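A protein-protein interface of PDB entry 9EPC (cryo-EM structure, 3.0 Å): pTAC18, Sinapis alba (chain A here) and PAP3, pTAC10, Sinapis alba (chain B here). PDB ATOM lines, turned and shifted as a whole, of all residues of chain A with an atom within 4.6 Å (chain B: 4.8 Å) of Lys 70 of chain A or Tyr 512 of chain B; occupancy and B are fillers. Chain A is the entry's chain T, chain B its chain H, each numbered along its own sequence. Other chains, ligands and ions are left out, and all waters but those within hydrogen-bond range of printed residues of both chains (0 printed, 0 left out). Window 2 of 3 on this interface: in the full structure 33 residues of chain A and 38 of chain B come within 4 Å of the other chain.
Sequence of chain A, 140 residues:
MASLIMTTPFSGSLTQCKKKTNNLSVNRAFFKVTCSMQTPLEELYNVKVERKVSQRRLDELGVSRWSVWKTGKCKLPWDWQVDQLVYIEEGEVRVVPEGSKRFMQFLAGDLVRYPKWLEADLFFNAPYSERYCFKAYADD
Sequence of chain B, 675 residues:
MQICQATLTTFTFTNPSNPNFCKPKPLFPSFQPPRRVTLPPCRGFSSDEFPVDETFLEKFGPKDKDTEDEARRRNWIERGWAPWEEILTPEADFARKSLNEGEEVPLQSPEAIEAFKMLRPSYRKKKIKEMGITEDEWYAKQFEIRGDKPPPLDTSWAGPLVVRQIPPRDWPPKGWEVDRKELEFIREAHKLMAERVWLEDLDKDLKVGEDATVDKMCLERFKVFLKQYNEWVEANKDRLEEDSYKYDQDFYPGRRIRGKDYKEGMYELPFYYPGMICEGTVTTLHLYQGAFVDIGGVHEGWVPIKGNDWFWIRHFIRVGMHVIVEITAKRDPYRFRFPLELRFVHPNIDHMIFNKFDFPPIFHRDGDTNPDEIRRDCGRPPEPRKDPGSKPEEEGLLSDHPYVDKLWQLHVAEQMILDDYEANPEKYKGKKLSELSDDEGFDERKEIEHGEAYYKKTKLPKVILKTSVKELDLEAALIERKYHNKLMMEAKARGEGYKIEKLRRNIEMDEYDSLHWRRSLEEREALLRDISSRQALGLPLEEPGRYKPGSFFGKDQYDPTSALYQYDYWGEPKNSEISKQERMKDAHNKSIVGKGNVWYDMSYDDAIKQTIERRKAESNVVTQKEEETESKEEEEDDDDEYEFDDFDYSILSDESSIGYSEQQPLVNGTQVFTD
A ring nitrogen (NE2) of His 401 of chain B is in hydrogen-bond range of the backbone carbonyl oxygen (O) of Lys 70 of chain A, 3.5 Å away.
ND1 of His 401 of chain B sits at hydrogen-bond distance from N of Tyr 403 of chain B, at 3.0 Å. The side-chain carboxylate (OD1) of Asp 513 of chain B sits close to the backbone NH (N) of His 401 of chain B (3.2 Å). The backbone carbonyl oxygen of Thr 71 of chain A is in hydrogen-bond range of the backbone NH of Tyr 128 of chain A.
Val 68 of chain A touches Leu 515 of chain B. Trp 69 of chain A touches His 401 of chain B (CZ2 to NE2, 3.8 Å). Trp 69 of chain A touches Leu 515 of chain B. NE1 of Trp 69 of chain A touches CD2 of His 516 of chain B (3.6 Å). Lys 70 of chain A touches Tyr 512 of chain B. Lys 70 of chain A touches Leu 515 of chain B. Thr 71 of chain A touches His 401 of chain B (OG1 to CE1, 3.1 Å). Thr 71 of chain A touches Tyr 403 of chain B (OG1 to CB, 3.3 Å).
Of the printed residues of chain B, Val 68 of chain A touches Leu 515 (3.3 Å). Of the printed residues of chain B, Trp 69 of chain A touches His 401, Leu 515 and His 516. Of the printed residues of chain B, Lys 70 of chain A touches His 401 (3.5 Å), Tyr 512 (3.2 Å) and Leu 515 (3.7 Å). Of the printed residues of chain A, His 401 of chain B touches Trp 69, Lys 70 and Thr 71. Glu 511 of chain B touches none of the printed residues of chain A. Of chain A, only Lys 70 comes within 4 Å of Tyr 512 of chain B. The nearest residue of chain B that does not touch Lys 70 of chain A is Glu 511 of chain B (4.2 Å). The nearest printed residue of chain B that does not touch Thr 71 of chain A is Tyr 512 of chain B (4.8 Å).
Hydrophobic or aromatic side chains of chain B that line the printed part of chain A: His 401, Tyr 403, Tyr 512, Leu 515 and His 516.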
ATOM      1  N   VAL A  68      35.560  13.723  24.245  1.00  0.00           N
ATOM      2  CA  VAL A  68      34.117  13.830  24.422  1.00  0.00           C
ATOM      3  C   VAL A  68      33.593  12.513  24.972  1.00  0.00           C
ATOM      4  O   VAL A  68      33.944  11.438  24.473  1.00  0.00           O
ATOM      5  CB  VAL A  68      33.420  14.187  23.098  1.00  0.00           C
ATOM      6  CG1 VAL A  68      31.920  14.321  23.307  1.00  0.00           C
ATOM      7  CG2 VAL A  68      34.002  15.468  22.526  1.00  0.00           C
ATOM      8  N   TRP A  69      32.757  12.595  26.005  1.00  0.00           N
ATOM      9  CA  TRP A  69      32.122  11.426  26.603  1.00  0.00           C
ATOM     10  C   TRP A  69      30.627  11.699  26.684  1.00  0.00           C
ATOM     11  O   TRP A  69      30.186  12.527  27.487  1.00  0.00           O
ATOM     12  CB  TRP A  69      32.703  11.128  27.982  1.00  0.00           C
ATOM     13  CG  TRP A  69      32.192   9.870  28.591  1.00  0.00           C
ATOM     14  CD1 TRP A  69      32.644   8.606  28.362  1.00  0.00           C
ATOM     15  CD2 TRP A  69      31.132   9.751  29.543  1.00  0.00           C
ATOM     16  NE1 TRP A  69      31.929   7.705  29.110  1.00  0.00           N
ATOM     17  CE2 TRP A  69      30.995   8.385  29.845  1.00  0.00           C
ATOM     18  CE3 TRP A  69      30.285  10.668  30.170  1.00  0.00           C
ATOM     19  CZ2 TRP A  69      30.045   7.912  30.742  1.00  0.00           C
ATOM     20  CZ3 TRP A  69      29.345  10.198  31.061  1.00  0.00           C
ATOM     21  CH2 TRP A  69      29.231   8.833  31.339  1.00  0.00           C
ATOM     22  N   LYS A  70      29.851  10.998  25.862  1.00  0.00           N
ATOM     23  CA  LYS A  70      28.427  11.251  25.703  1.00  0.00           C
ATOM     24  C   LYS A  70      27.627  10.035  26.146  1.00  0.00           C
ATOM     25  O   LYS A  70      28.005   8.894  25.861  1.00  0.00           O
ATOM     26  CB  LYS A  70      28.104  11.600  24.247  1.00  0.00           C
ATOM     27  CG  LYS A  70      26.626  11.706  23.929  1.00  0.00           C
ATOM     28  CD  LYS A  70      26.406  12.415  22.602  1.00  0.00           C
ATOM     29  CE  LYS A  70      27.293  11.843  21.506  1.00  0.00           C
ATOM     30  NZ  LYS A  70      27.017  10.404  21.248  1.00  0.00           N
ATOM     31  N   THR A  71      26.522  10.282  26.846  1.00  0.00           N
ATOM     32  CA  THR A  71      25.688   9.203  27.354  1.00  0.00           C
ATOM     33  C   THR A  71      24.257   9.691  27.505  1.00  0.00           C
ATOM     34  O   THR A  71      23.980  10.893  27.487  1.00  0.00           O
ATOM     35  CB  THR A  71      26.197   8.678  28.699  1.00  0.00           C
ATOM     36  OG1 THR A  71      25.402   7.556  29.103  1.00  0.00           O
ATOM     37  CG2 THR A  71      26.091   9.757  29.757  1.00  0.00           C
ATOM     38  N   TYR A 128      23.401  13.319  27.687  1.00  0.00           N
ATOM     39  CA  TYR A 128      24.422  14.117  28.348  1.00  0.00           C
ATOM     40  C   TYR A 128      25.772  13.847  27.706  1.00  0.00           C
ATOM     41  O   TYR A 128      26.136  12.688  27.482  1.00  0.00           O
ATOM     42  CB  TYR A 128      24.460  13.793  29.844  1.00  0.00           C
ATOM     43  CG  TYR A 128      25.763  14.108  30.538  1.00  0.00           C
ATOM     44  CD1 TYR A 128      26.017  15.375  31.035  1.00  0.00           C
ATOM     45  CD2 TYR A 128      26.728  13.128  30.722  1.00  0.00           C
ATOM     46  CE1 TYR A 128      27.201  15.662  31.681  1.00  0.00           C
ATOM     47  CE2 TYR A 128      27.915  13.407  31.365  1.00  0.00           C
ATOM     48  CZ  TYR A 128      28.146  14.676  31.843  1.00  0.00           C
ATOM     49  OH  TYR A 128      29.324  14.964  32.488  1.00  0.00           O
ATOM     50  N   SER A 129      26.512  14.912  27.416  1.00  0.00           N
ATOM     51  CA  SER A 129      27.860  14.806  26.887  1.00  0.00           C
ATOM     52  C   SER A 129      28.775  15.730  27.671  1.00  0.00           C
ATOM     53  O   SER A 129      28.366  16.805  28.116  1.00  0.00           O
ATOM     54  CB  SER A 129      27.923  15.157  25.395  1.00  0.00           C
ATOM     55  OG  SER A 129      27.725  16.542  25.189  1.00  0.00           O
ATOM     56  N   HIS B 401      30.222   0.506  28.848  1.00  0.00           N
ATOM     57  CA  HIS B 401      29.482   1.752  28.984  1.00  0.00           C
ATOM     58  C   HIS B 401      28.101   1.451  29.549  1.00  0.00           C
ATOM     59  O   HIS B 401      27.379   0.621  28.983  1.00  0.00           O
ATOM     60  CB  HIS B 401      29.368   2.461  27.642  1.00  0.00           C
ATOM     61  CG  HIS B 401      28.896   3.876  27.749  1.00  0.00           C
ATOM     62  ND1 HIS B 401      27.619   4.207  28.143  1.00  0.00           N
ATOM     63  CD2 HIS B 401      29.532   5.048  27.514  1.00  0.00           C
ATOM     64  CE1 HIS B 401      27.488   5.521  28.146  1.00  0.00           C
ATOM     65  NE2 HIS B 401      28.635   6.055  27.768  1.00  0.00           N
ATOM     66  N   TYR B 403      25.239   3.008  29.562  1.00  0.00           N
ATOM     67  CA  TYR B 403      24.078   3.307  28.734  1.00  0.00           C
ATOM     68  C   TYR B 403      23.846   2.254  27.661  1.00  0.00           C
ATOM     69  O   TYR B 403      22.717   2.124  27.177  1.00  0.00           O
ATOM     70  CB  TYR B 403      24.226   4.682  28.086  1.00  0.00           C
ATOM     71  CG  TYR B 403      23.024   5.097  27.274  1.00  0.00           C
ATOM     72  CD1 TYR B 403      21.833   5.444  27.894  1.00  0.00           C
ATOM     73  CD2 TYR B 403      23.077   5.137  25.890  1.00  0.00           C
ATOM     74  CE1 TYR B 403      20.729   5.821  27.159  1.00  0.00           C
ATOM     75  CE2 TYR B 403      21.979   5.514  25.145  1.00  0.00           C
ATOM     76  CZ  TYR B 403      20.808   5.855  25.785  1.00  0.00           C
ATOM     77  OH  TYR B 403      19.708   6.231  25.050  1.00  0.00           O
ATOM     78  N   VAL B 404      24.881   1.500  27.284  1.00  0.00           N
ATOM     79  CA  VAL B 404      24.719   0.474  26.258  1.00  0.00           C
ATOM     80  C   VAL B 404      23.699  -0.563  26.703  1.00  0.00           C
ATOM     81  O   VAL B 404      22.880  -1.033  25.904  1.00  0.00           O
ATOM     82  CB  VAL B 404      26.077  -0.171  25.928  1.00  0.00           C
ATOM     83  CG1 VAL B 404      25.899  -1.297  24.930  1.00  0.00           C
ATOM     84  CG2 VAL B 404      27.033   0.872  25.383  1.00  0.00           C
ATOM     85  N   LEU B 407      20.653   1.111  26.210  1.00  0.00           N
ATOM     86  CA  LEU B 407      20.512   1.243  24.766  1.00  0.00           C
ATOM     87  C   LEU B 407      20.185  -0.091  24.116  1.00  0.00           C
ATOM     88  O   LEU B 407      19.506  -0.131  23.084  1.00  0.00           O
ATOM     89  CB  LEU B 407      21.791   1.826  24.168  1.00  0.00           C
ATOM     90  CG  LEU B 407      21.711   2.298  22.722  1.00  0.00           C
ATOM     91  CD1 LEU B 407      20.628   3.350  22.582  1.00  0.00           C
ATOM     92  CD2 LEU B 407      23.053   2.848  22.284  1.00  0.00           C
ATOM     93  N   GLU B 508      26.329   2.046  17.000  1.00  0.00           N
ATOM     94  CA  GLU B 508      26.302   3.176  17.921  1.00  0.00           C
ATOM     95  C   GLU B 508      26.613   2.736  19.344  1.00  0.00           C
ATOM     96  O   GLU B 508      27.014   3.560  20.174  1.00  0.00           O
ATOM     97  CB  GLU B 508      24.952   3.889  17.863  1.00  0.00           C
ATOM     98  CG  GLU B 508      23.902   3.318  18.793  1.00  0.00           C
ATOM     99  CD  GLU B 508      22.685   4.212  18.909  1.00  0.00           C
ATOM    100  OE1 GLU B 508      22.739   5.358  18.415  1.00  0.00           O
ATOM    101  OE2 GLU B 508      21.675   3.771  19.494  1.00  0.00           O
ATOM    102  N   MET B 509      26.429   1.451  19.648  1.00  0.00           N
ATOM    103  CA  MET B 509      26.929   0.926  20.912  1.00  0.00           C
ATOM    104  C   MET B 509      28.451   0.881  20.909  1.00  0.00           C
ATOM    105  O   MET B 509      29.089   1.119  21.941  1.00  0.00           O
ATOM    106  CB  MET B 509      26.354  -0.467  21.171  1.00  0.00           C
ATOM    107  CG  MET B 509      24.837  -0.534  21.252  1.00  0.00           C
ATOM    108  SD  MET B 509      24.260  -2.243  21.178  1.00  0.00           S
ATOM    109  CE  MET B 509      22.485  -2.039  21.272  1.00  0.00           C
ATOM    110  N   ASP B 510      29.044   0.587  19.750  1.00  0.00           N
ATOM    111  CA  ASP B 510      30.496   0.502  19.651  1.00  0.00           C
ATOM    112  C   ASP B 510      31.150   1.834  19.986  1.00  0.00           C
ATOM    113  O   ASP B 510      32.136   1.880  20.733  1.00  0.00           O
ATOM    114  CB  ASP B 510      30.888   0.049  18.245  1.00  0.00           C
ATOM    115  CG  ASP B 510      32.259  -0.594  18.194  1.00  0.00           C
ATOM    116  OD1 ASP B 510      33.101  -0.290  19.064  1.00  0.00           O
ATOM    117  OD2 ASP B 510      32.489  -1.407  17.276  1.00  0.00           O
ATOM    118  N   GLU B 511      30.616   2.933  19.449  1.00  0.00           N
ATOM    119  CA  GLU B 511      31.192   4.239  19.744  1.00  0.00           C
ATOM    120  C   GLU B 511      30.949   4.643  21.192  1.00  0.00           C
ATOM    121  O   GLU B 511      31.812   5.282  21.804  1.00  0.00           O
ATOM    122  CB  GLU B 511      30.642   5.292  18.781  1.00  0.00           C
ATOM    123  CG  GLU B 511      29.130   5.394  18.730  1.00  0.00           C
ATOM    124  CD  GLU B 511      28.572   6.366  19.750  1.00  0.00           C
ATOM    125  OE1 GLU B 511      29.368   7.096  20.376  1.00  0.00           O
ATOM    126  OE2 GLU B 511      27.336   6.401  19.924  1.00  0.00           O
ATOM    127  N   TYR B 512      29.794   4.284  21.756  1.00  0.00           N
ATOM    128  CA  TYR B 512      29.559   4.557  23.170  1.00  0.00           C
ATOM    129  C   TYR B 512      30.550   3.802  24.044  1.00  0.00           C
ATOM    130  O   TYR B 512      31.091   4.358  25.006  1.00  0.00           O
ATOM    131  CB  TYR B 512      28.123   4.203  23.548  1.00  0.00           C
ATOM    132  CG  TYR B 512      27.145   5.329  23.314  1.00  0.00           C
ATOM    133  CD1 TYR B 512      27.591   6.625  23.099  1.00  0.00           C
ATOM    134  CD2 TYR B 512      25.778   5.099  23.316  1.00  0.00           C
ATOM    135  CE1 TYR B 512      26.703   7.658  22.888  1.00  0.00           C
ATOM    136  CE2 TYR B 512      24.882   6.128  23.105  1.00  0.00           C
ATOM    137  CZ  TYR B 512      25.349   7.405  22.892  1.00  0.00           C
ATOM    138  OH  TYR B 512      24.459   8.431  22.680  1.00  0.00           O
ATOM    139  N   ASP B 513      30.805   2.532  23.724  1.00  0.00           N
ATOM    140  CA  ASP B 513      31.885   1.815  24.392  1.00  0.00           C
ATOM    141  C   ASP B 513      33.230   2.455  24.082  1.00  0.00           C
ATOM    142  O   ASP B 513      34.091   2.567  24.962  1.00  0.00           O
ATOM    143  CB  ASP B 513      31.880   0.345  23.980  1.00  0.00           C
ATOM    144  CG  ASP B 513      30.849  -0.466  24.732  1.00  0.00           C
ATOM    145  OD1 ASP B 513      30.210   0.091  25.648  1.00  0.00           O
ATOM    146  OD2 ASP B 513      30.678  -1.661  24.412  1.00  0.00           O
ATOM    147  N   SER B 514      33.425   2.886  22.833  1.00  0.00           N
ATOM    148  CA  SER B 514      34.676   3.539  22.464  1.00  0.00           C
ATOM    149  C   SER B 514      34.886   4.817  23.265  1.00  0.00           C
ATOM    150  O   SER B 514      35.997   5.087  23.736  1.00  0.00           O
ATOM    151  CB  SER B 514      34.690   3.837  20.966  1.00  0.00           C
ATOM    152  OG  SER B 514      35.884   4.500  20.592  1.00  0.00           O
ATOM    153  N   LEU B 515      33.831   5.617  23.430  1.00  0.00           N
ATOM    154  CA  LEU B 515      33.944   6.820  24.248  1.00  0.00           C
ATOM    155  C   LEU B 515      34.265   6.464  25.693  1.00  0.00           C
ATOM    156  O   LEU B 515      35.130   7.086  26.320  1.00  0.00           O
ATOM    157  CB  LEU B 515      32.655   7.636  24.168  1.00  0.00           C
ATOM    158  CG  LEU B 515      32.319   8.254  22.812  1.00  0.00           C
ATOM    159  CD1 LEU B 515      31.084   9.134  22.920  1.00  0.00           C
ATOM    160  CD2 LEU B 515      33.502   9.038  22.268  1.00  0.00           C
ATOM    161  N   HIS B 516      33.578   5.458  26.238  1.00  0.00           N
ATOM    162  CA  HIS B 516      33.858   5.039  27.605  1.00  0.00           C
ATOM    163  C   HIS B 516      35.245   4.424  27.717  1.00  0.00           C
ATOM    164  O   HIS B 516      35.957   4.656  28.701  1.00  0.00           O
ATOM    165  CB  HIS B 516      32.793   4.055  28.082  1.00  0.00           C
ATOM    166  CG  HIS B 516      32.814   3.815  29.558  1.00  0.00           C
ATOM    167  ND1 HIS B 516      33.525   2.785  30.135  1.00  0.00           N
ATOM    168  CD2 HIS B 516      32.209   4.471  30.576  1.00  0.00           C
ATOM    169  CE1 HIS B 516      33.357   2.818  31.444  1.00  0.00           C
ATOM    170  NE2 HIS B 516      32.563   3.831  31.738  1.00  0.00           N
